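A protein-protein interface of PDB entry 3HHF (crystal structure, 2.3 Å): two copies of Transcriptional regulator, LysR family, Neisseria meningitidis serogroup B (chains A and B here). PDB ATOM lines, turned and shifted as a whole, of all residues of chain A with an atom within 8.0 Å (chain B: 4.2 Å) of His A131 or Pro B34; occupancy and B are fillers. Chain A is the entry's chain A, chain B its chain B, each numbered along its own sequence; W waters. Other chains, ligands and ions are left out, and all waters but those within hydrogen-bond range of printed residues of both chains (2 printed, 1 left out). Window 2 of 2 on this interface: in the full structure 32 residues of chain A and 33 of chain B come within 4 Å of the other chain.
Water W2 bridges OG1 of Thr A133 (2.9 Å) and O of Arg B37 (3.5 Å).
Water W1 lies within hydrogen-bond range of the backbone carbonyl oxygen of Pro A130 (3.0 Å), the backbone carbonyl oxygen of His A131 (3.2 Å) and the guanidinium group of Arg B37 (3.3 Å).
Among the printed residues, merely in contact across the chains: His A131 with Arg B37 (3.2 Å), His A131 with Pro B34 (3.3 Å), Phe A132 with Ile B36 (3.7 Å) and Phe A132 with Asn B30 (3.9 Å).
The side-chain amide nitrogen (ND2) of Asn B30 lies within hydrogen-bond range of the side-chain amide oxygen (OE1) of Gln A103 (3.1 Å).
NE2 of His A131 is in hydrogen-bond range of OD1 of Asn B30.
His A102 touches none of the printed residues of chain B.
Ser A129 touches none of the printed residues of chain B.
Of chain B, only Asn B30 (3.1 Å), Pro B34 (3.3 Å) and Arg B37 (3.2 Å) come within 4 Å of His A131.
Of the printed residues of chain B, Phe A132 touches Asn B30 and Ile B36.
Of the printed residues of chain A, Asn B30 touches Gln A103, His A131 and Phe A132.
Pro B34 touches just one residue of chain A: His A131.
Of the printed residues of chain A, Arg B37 touches His A131.
The nearest printed residue of chain B that does not touch His A131 is Ile B36 (4.2 Å).
The nearest residue of chain A that does not touch Pro B34 is Gln A103 (5.4 Å).
No position is printed for both chains.
Of the 6 pairs that touch across the chains among the printed residues, none has its exchanged pair printed and touching as well.
N of Gln A103 sits at hydrogen-bond distance from OH of Tyr A86 (2.9 Å).
The backbone carbonyl oxygen (O) of Cys A148 lies close to the side-chain amide oxygen (OE1) of Gln A103, at 2.9 Å.
The backbone NH (N) of Ile A150 sits at hydrogen-bond distance from the backbone carbonyl oxygen (O) of Gln A103 (2.8 Å).
N of His A131 is in hydrogen-bond range of O of Cys A104 (2.7 Å).
N of Gly A106 is in hydrogen-bond range of O of Phe A132, 3.0 Å away.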
ATOM      1  N   TYR A  86      12.946  -6.973   7.243  1.00  0.00           N
ATOM      2  CA  TYR A  86      13.436  -7.153   5.879  1.00  0.00           C
ATOM      3  C   TYR A  86      12.269  -7.325   4.915  1.00  0.00           C
ATOM      4  O   TYR A  86      12.254  -6.744   3.839  1.00  0.00           O
ATOM      5  CB  TYR A  86      14.365  -8.373   5.764  1.00  0.00           C
ATOM      6  CG  TYR A  86      14.758  -8.640   4.326  1.00  0.00           C
ATOM      7  CD1 TYR A  86      14.028  -9.515   3.529  1.00  0.00           C
ATOM      8  CD2 TYR A  86      15.823  -7.964   3.749  1.00  0.00           C
ATOM      9  CE1 TYR A  86      14.364  -9.724   2.200  1.00  0.00           C
ATOM     10  CE2 TYR A  86      16.171  -8.168   2.430  1.00  0.00           C
ATOM     11  CZ  TYR A  86      15.443  -9.049   1.657  1.00  0.00           C
ATOM     12  OH  TYR A  86      15.807  -9.236   0.343  1.00  0.00           O
ATOM     13  N   HIS A 102      16.002 -10.860  -4.276  1.00  0.00           N
ATOM     14  CA  HIS A 102      16.250 -10.579  -2.855  1.00  0.00           C
ATOM     15  C   HIS A 102      17.702 -10.752  -2.449  1.00  0.00           C
ATOM     16  O   HIS A 102      18.505 -11.323  -3.182  1.00  0.00           O
ATOM     17  CB  HIS A 102      15.348 -11.446  -1.970  1.00  0.00           C
ATOM     18  CG  HIS A 102      13.933 -10.970  -1.929  1.00  0.00           C
ATOM     19  ND1 HIS A 102      12.935 -11.546  -2.686  1.00  0.00           N
ATOM     20  CD2 HIS A 102      13.357  -9.948  -1.256  1.00  0.00           C
ATOM     21  CE1 HIS A 102      11.801 -10.903  -2.467  1.00  0.00           C
ATOM     22  NE2 HIS A 102      12.030  -9.932  -1.601  1.00  0.00           N
ATOM     23  N   GLN A 103      18.030 -10.232  -1.273  1.00  0.00           N
ATOM     24  CA  GLN A 103      19.354 -10.411  -0.700  1.00  0.00           C
ATOM     25  C   GLN A 103      19.399 -11.734   0.033  1.00  0.00           C
ATOM     26  O   GLN A 103      18.790 -11.878   1.078  1.00  0.00           O
ATOM     27  CB  GLN A 103      19.681  -9.275   0.259  1.00  0.00           C
ATOM     28  CG  GLN A 103      19.900  -7.961  -0.442  1.00  0.00           C
ATOM     29  CD  GLN A 103      20.186  -6.831   0.515  1.00  0.00           C
ATOM     30  OE1 GLN A 103      19.917  -6.928   1.716  1.00  0.00           O
ATOM     31  NE2 GLN A 103      20.734  -5.739  -0.014  1.00  0.00           N
ATOM     32  N   CYS A 104      20.112 -12.699  -0.539  1.00  0.00           N
ATOM     33  CA  CYS A 104      20.314 -14.005   0.079  1.00  0.00           C
ATOM     34  C   CYS A 104      21.732 -14.100   0.618  1.00  0.00           C
ATOM     35  O   CYS A 104      22.689 -13.847  -0.107  1.00  0.00           O
ATOM     36  CB  CYS A 104      20.064 -15.121  -0.931  1.00  0.00           C
ATOM     37  SG  CYS A 104      18.408 -15.068  -1.613  1.00  0.00           S
ATOM     38  N   LEU A 105      21.843 -14.453   1.899  1.00  0.00           N
ATOM     39  CA  LEU A 105      23.119 -14.532   2.604  1.00  0.00           C
ATOM     40  C   LEU A 105      23.517 -15.993   2.712  1.00  0.00           C
ATOM     41  O   LEU A 105      22.668 -16.860   2.881  1.00  0.00           O
ATOM     42  CB  LEU A 105      23.000 -13.922   4.009  1.00  0.00           C
ATOM     43  CG  LEU A 105      22.140 -12.666   4.180  1.00  0.00           C
ATOM     44  CD1 LEU A 105      22.309 -12.131   5.583  1.00  0.00           C
ATOM     45  CD2 LEU A 105      22.491 -11.596   3.147  1.00  0.00           C
ATOM     46  N   GLY A 106      24.812 -16.267   2.627  1.00  0.00           N
ATOM     47  CA  GLY A 106      25.296 -17.644   2.575  1.00  0.00           C
ATOM     48  C   GLY A 106      26.596 -17.867   3.314  1.00  0.00           C
ATOM     49  O   GLY A 106      27.118 -16.965   3.972  1.00  0.00           O
ATOM     50  N   ILE A 128      22.104 -20.140  -4.587  1.00  0.00           N
ATOM     51  CA  ILE A 128      22.057 -18.691  -4.440  1.00  0.00           C
ATOM     52  C   ILE A 128      23.382 -18.044  -4.811  1.00  0.00           C
ATOM     53  O   ILE A 128      24.408 -18.711  -4.887  1.00  0.00           O
ATOM     54  CB  ILE A 128      21.635 -18.259  -3.003  1.00  0.00           C
ATOM     55  CG1 ILE A 128      22.696 -18.637  -1.958  1.00  0.00           C
ATOM     56  CG2 ILE A 128      20.276 -18.853  -2.656  1.00  0.00           C
ATOM     57  CD1 ILE A 128      22.618 -17.834  -0.683  1.00  0.00           C
ATOM     58  N   SER A 129      23.331 -16.742  -5.065  1.00  0.00           N
ATOM     59  CA  SER A 129      24.524 -15.912  -5.176  1.00  0.00           C
ATOM     60  C   SER A 129      24.572 -15.066  -3.910  1.00  0.00           C
ATOM     61  O   SER A 129      23.858 -14.073  -3.815  1.00  0.00           O
ATOM     62  CB  SER A 129      24.445 -15.022  -6.419  1.00  0.00           C
ATOM     63  OG  SER A 129      24.334 -15.807  -7.598  1.00  0.00           O
ATOM     64  N   PRO A 130      25.383 -15.470  -2.916  1.00  0.00           N
ATOM     65  CA  PRO A 130      25.311 -14.778  -1.630  1.00  0.00           C
ATOM     66  C   PRO A 130      25.655 -13.296  -1.717  1.00  0.00           C
ATOM     67  O   PRO A 130      26.622 -12.924  -2.375  1.00  0.00           O
ATOM     68  CB  PRO A 130      26.328 -15.526  -0.756  1.00  0.00           C
ATOM     69  CG  PRO A 130      27.189 -16.268  -1.689  1.00  0.00           C
ATOM     70  CD  PRO A 130      26.378 -16.558  -2.903  1.00  0.00           C
ATOM     71  N   HIS A 131      24.849 -12.460  -1.068  1.00  0.00           N
ATOM     72  CA  HIS A 131      25.166 -11.043  -0.947  1.00  0.00           C
ATOM     73  C   HIS A 131      26.191 -10.849   0.166  1.00  0.00           C
ATOM     74  O   HIS A 131      27.264 -10.283  -0.065  1.00  0.00           O
ATOM     75  CB  HIS A 131      23.915 -10.203  -0.673  1.00  0.00           C
ATOM     76  CG  HIS A 131      24.197  -8.734  -0.600  1.00  0.00           C
ATOM     77  ND1 HIS A 131      24.952  -8.077  -1.549  1.00  0.00           N
ATOM     78  CD2 HIS A 131      23.843  -7.798   0.313  1.00  0.00           C
ATOM     79  CE1 HIS A 131      25.048  -6.800  -1.227  1.00  0.00           C
ATOM     80  NE2 HIS A 131      24.382  -6.604  -0.103  1.00  0.00           N
ATOM     81  N   PHE A 132      25.838 -11.305   1.368  1.00  0.00           N
ATOM     82  CA  PHE A 132      26.789 -11.420   2.471  1.00  0.00           C
ATOM     83  C   PHE A 132      27.159 -12.886   2.636  1.00  0.00           C
ATOM     84  O   PHE A 132      26.362 -13.772   2.317  1.00  0.00           O
ATOM     85  CB  PHE A 132      26.210 -10.892   3.797  1.00  0.00           C
ATOM     86  CG  PHE A 132      26.045  -9.388   3.867  1.00  0.00           C
ATOM     87  CD1 PHE A 132      26.614  -8.533   2.915  1.00  0.00           C
ATOM     88  CD2 PHE A 132      25.333  -8.822   4.924  1.00  0.00           C
ATOM     89  CE1 PHE A 132      26.454  -7.152   3.009  1.00  0.00           C
ATOM     90  CE2 PHE A 132      25.173  -7.442   5.027  1.00  0.00           C
ATOM     91  CZ  PHE A 132      25.737  -6.608   4.069  1.00  0.00           C
ATOM     92  N   THR A 133      28.376 -13.133   3.116  1.00  0.00           N
ATOM     93  CA  THR A 133      28.803 -14.480   3.466  1.00  0.00           C
ATOM     94  C   THR A 133      29.252 -14.491   4.919  1.00  0.00           C
ATOM     95  O   THR A 133      29.509 -13.439   5.503  1.00  0.00           O
ATOM     96  CB  THR A 133      29.918 -15.028   2.519  1.00  0.00           C
ATOM     97  OG1 THR A 133      31.026 -14.124   2.462  1.00  0.00           O
ATOM     98  CG2 THR A 133      29.379 -15.236   1.101  1.00  0.00           C
ATOM     99  N   ALA A 134      29.288 -15.679   5.513  1.00  0.00           N
ATOM    100  CA  ALA A 134      29.766 -15.850   6.881  1.00  0.00           C
ATOM    101  C   ALA A 134      30.314 -17.260   7.085  1.00  0.00           C
ATOM    102  O   ALA A 134      29.975 -18.177   6.332  1.00  0.00           O
ATOM    103  CB  ALA A 134      28.655 -15.547   7.878  1.00  0.00           C
ATOM    104  N   LEU A 143      22.700 -11.922  11.275  1.00  0.00           N
ATOM    105  CA  LEU A 143      22.461 -11.088  10.094  1.00  0.00           C
ATOM    106  C   LEU A 143      20.993 -11.129   9.661  1.00  0.00           C
ATOM    107  O   LEU A 143      20.412 -10.099   9.332  1.00  0.00           O
ATOM    108  CB  LEU A 143      23.355 -11.533   8.929  1.00  0.00           C
ATOM    109  CG  LEU A 143      24.863 -11.324   9.105  1.00  0.00           C
ATOM    110  CD1 LEU A 143      25.644 -12.017   8.003  1.00  0.00           C
ATOM    111  CD2 LEU A 143      25.204  -9.847   9.162  1.00  0.00           C
ATOM    112  N   CYS A 148      19.215  -8.242   7.219  1.00  0.00           N
ATOM    113  CA  CYS A 148      20.176  -8.173   6.123  1.00  0.00           C
ATOM    114  C   CYS A 148      19.753  -9.017   4.925  1.00  0.00           C
ATOM    115  O   CYS A 148      20.325  -8.881   3.841  1.00  0.00           O
ATOM    116  CB  CYS A 148      21.570  -8.614   6.585  1.00  0.00           C
ATOM    117  SG  CYS A 148      22.362  -7.478   7.707  1.00  0.00           S
ATOM    118  N   GLY A 149      18.775  -9.896   5.118  1.00  0.00           N
ATOM    119  CA  GLY A 149      18.253 -10.684   4.014  1.00  0.00           C
ATOM    120  C   GLY A 149      17.735 -12.050   4.404  1.00  0.00           C
ATOM    121  O   GLY A 149      17.446 -12.321   5.570  1.00  0.00           O
ATOM    122  N   ILE A 150      17.642 -12.907   3.398  1.00  0.00           N
ATOM    123  CA  ILE A 150      17.068 -14.233   3.518  1.00  0.00           C
ATOM    124  C   ILE A 150      18.192 -15.241   3.699  1.00  0.00           C
ATOM    125  O   ILE A 150      19.210 -15.179   3.006  1.00  0.00           O
ATOM    126  CB  ILE A 150      16.254 -14.590   2.249  1.00  0.00           C
ATOM    127  CG1 ILE A 150      15.197 -13.510   1.988  1.00  0.00           C
ATOM    128  CG2 ILE A 150      15.623 -15.974   2.380  1.00  0.00           C
ATOM    129  CD1 ILE A 150      14.322 -13.753   0.775  1.00  0.00           C
ATOM    130  N   ASN B  30      24.722  -1.772   5.006  1.00  0.00           N
ATOM    131  CA  ASN B  30      24.144  -2.248   3.746  1.00  0.00           C
ATOM    132  C   ASN B  30      23.291  -1.187   3.039  1.00  0.00           C
ATOM    133  O   ASN B  30      23.369  -1.036   1.821  1.00  0.00           O
ATOM    134  CB  ASN B  30      23.307  -3.509   4.003  1.00  0.00           C
ATOM    135  CG  ASN B  30      22.777  -4.137   2.728  1.00  0.00           C
ATOM    136  OD1 ASN B  30      23.526  -4.356   1.773  1.00  0.00           O
ATOM    137  ND2 ASN B  30      21.478  -4.437   2.711  1.00  0.00           N
ATOM    138  N   GLU B  31      22.479  -0.461   3.805  1.00  0.00           N
ATOM    139  CA  GLU B  31      21.672   0.642   3.269  1.00  0.00           C
ATOM    140  C   GLU B  31      22.527   1.805   2.761  1.00  0.00           C
ATOM    141  O   GLU B  31      22.174   2.450   1.778  1.00  0.00           O
ATOM    142  CB  GLU B  31      20.688   1.156   4.325  1.00  0.00           C
ATOM    143  CG  GLU B  31      19.571   0.172   4.644  1.00  0.00           C
ATOM    144  CD  GLU B  31      18.619   0.652   5.738  1.00  0.00           C
ATOM    145  OE1 GLU B  31      18.959   1.592   6.495  1.00  0.00           O
ATOM    146  OE2 GLU B  31      17.518   0.071   5.844  1.00  0.00           O
ATOM    147  N   ARG B  32      23.643   2.074   3.428  1.00  0.00           N
ATOM    148  CA  ARG B  32      24.536   3.159   3.024  1.00  0.00           C
ATOM    149  C   ARG B  32      25.433   2.759   1.845  1.00  0.00           C
ATOM    150  O   ARG B  32      25.643   3.547   0.925  1.00  0.00           O
ATOM    151  CB  ARG B  32      25.391   3.610   4.212  1.00  0.00           C
ATOM    152  CG  ARG B  32      26.084   4.952   4.003  1.00  0.00           C
ATOM    153  CD  ARG B  32      26.841   5.401   5.243  1.00  0.00           C
ATOM    154  NE  ARG B  32      25.966   5.538   6.406  1.00  0.00           N
ATOM    155  CZ  ARG B  32      26.379   5.864   7.631  1.00  0.00           C
ATOM    156  NH1 ARG B  32      25.498   5.954   8.623  1.00  0.00           N
ATOM    157  NH2 ARG B  32      27.666   6.105   7.876  1.00  0.00           N
ATOM    158  N   TYR B  33      25.967   1.540   1.891  1.00  0.00           N
ATOM    159  CA  TYR B  33      26.851   1.019   0.849  1.00  0.00           C
ATOM    160  C   TYR B  33      26.347  -0.348   0.383  1.00  0.00           C
ATOM    161  O   TYR B  33      26.910  -1.377   0.747  1.00  0.00           O
ATOM    162  CB  TYR B  33      28.285   0.897   1.377  1.00  0.00           C
ATOM    163  CG  TYR B  33      28.820   2.153   2.018  1.00  0.00           C
ATOM    164  CD1 TYR B  33      28.954   2.245   3.399  1.00  0.00           C
ATOM    165  CD2 TYR B  33      29.193   3.250   1.251  1.00  0.00           C
ATOM    166  CE1 TYR B  33      29.445   3.395   4.005  1.00  0.00           C
ATOM    167  CE2 TYR B  33      29.688   4.412   1.850  1.00  0.00           C
ATOM    168  CZ  TYR B  33      29.805   4.477   3.229  1.00  0.00           C
ATOM    169  OH  TYR B  33      30.293   5.617   3.830  1.00  0.00           O
ATOM    170  N   PRO B  34      25.269  -0.363  -0.419  1.00  0.00           N
ATOM    171  CA  PRO B  34      24.685  -1.632  -0.890  1.00  0.00           C
ATOM    172  C   PRO B  34      25.548  -2.473  -1.847  1.00  0.00           C
ATOM    173  O   PRO B  34      25.226  -3.635  -2.076  1.00  0.00           O
ATOM    174  CB  PRO B  34      23.387  -1.190  -1.584  1.00  0.00           C
ATOM    175  CG  PRO B  34      23.592   0.243  -1.921  1.00  0.00           C
ATOM    176  CD  PRO B  34      24.512   0.809  -0.896  1.00  0.00           C
ATOM    177  N   HIS B  35      26.619  -1.906  -2.392  1.00  0.00           N
ATOM    178  CA  HIS B  35      27.461  -2.623  -3.355  1.00  0.00           C
ATOM    179  C   HIS B  35      28.691  -3.269  -2.718  1.00  0.00           C
ATOM    180  O   HIS B  35      29.503  -3.874  -3.421  1.00  0.00           O
ATOM    181  CB  HIS B  35      27.890  -1.687  -4.489  1.00  0.00           C
ATOM    182  CG  HIS B  35      26.746  -0.978  -5.143  1.00  0.00           C
ATOM    183  ND1 HIS B  35      25.706  -1.649  -5.750  1.00  0.00           N
ATOM    184  CD2 HIS B  35      26.476   0.340  -5.283  1.00  0.00           C
ATOM    185  CE1 HIS B  35      24.844  -0.774  -6.235  1.00  0.00           C
ATOM    186  NE2 HIS B  35      25.286   0.441  -5.965  1.00  0.00           N
ATOM    187  N   ILE B  36      28.833  -3.135  -1.396  1.00  0.00           N
ATOM    188  CA  ILE B  36      29.907  -3.801  -0.663  1.00  0.00           C
ATOM    189  C   ILE B  36      29.360  -5.099  -0.075  1.00  0.00           C
ATOM    190  O   ILE B  36      28.395  -5.089   0.688  1.00  0.00           O
ATOM    191  CB  ILE B  36      30.491  -2.921   0.476  1.00  0.00           C
ATOM    192  CG1 ILE B  36      30.954  -1.563  -0.058  1.00  0.00           C
ATOM    193  CG2 ILE B  36      31.659  -3.637   1.157  1.00  0.00           C
ATOM    194  CD1 ILE B  36      31.426  -0.610   1.025  1.00  0.00           C
ATOM    195  N   ARG B  37      29.991  -6.208  -0.436  1.00  0.00           N
ATOM    196  CA  ARG B  37      29.546  -7.533  -0.035  1.00  0.00           C
ATOM    197  C   ARG B  37      30.361  -8.029   1.157  1.00  0.00           C
ATOM    198  O   ARG B  37      31.430  -8.618   0.997  1.00  0.00           O
ATOM    199  CB  ARG B  37      29.666  -8.497  -1.221  1.00  0.00           C
ATOM    200  CG  ARG B  37      28.838  -8.072  -2.425  1.00  0.00           C
ATOM    201  CD  ARG B  37      28.592  -9.220  -3.387  1.00  0.00           C
ATOM    202  NE  ARG B  37      29.831  -9.855  -3.825  1.00  0.00           N
ATOM    203  CZ  ARG B  37      30.665  -9.357  -4.738  1.00  0.00           C
ATOM    204  NH1 ARG B  37      30.422  -8.187  -5.333  1.00  0.00           N
ATOM    205  NH2 ARG B  37      31.763 -10.036  -5.059  1.00  0.00           N
HETATM  206  O   HOH W   1      29.418 -12.199  -1.535  1.00  0.00           O
HETATM  207  O   HOH W   2      30.850 -11.998   0.433  1.00  0.00           O
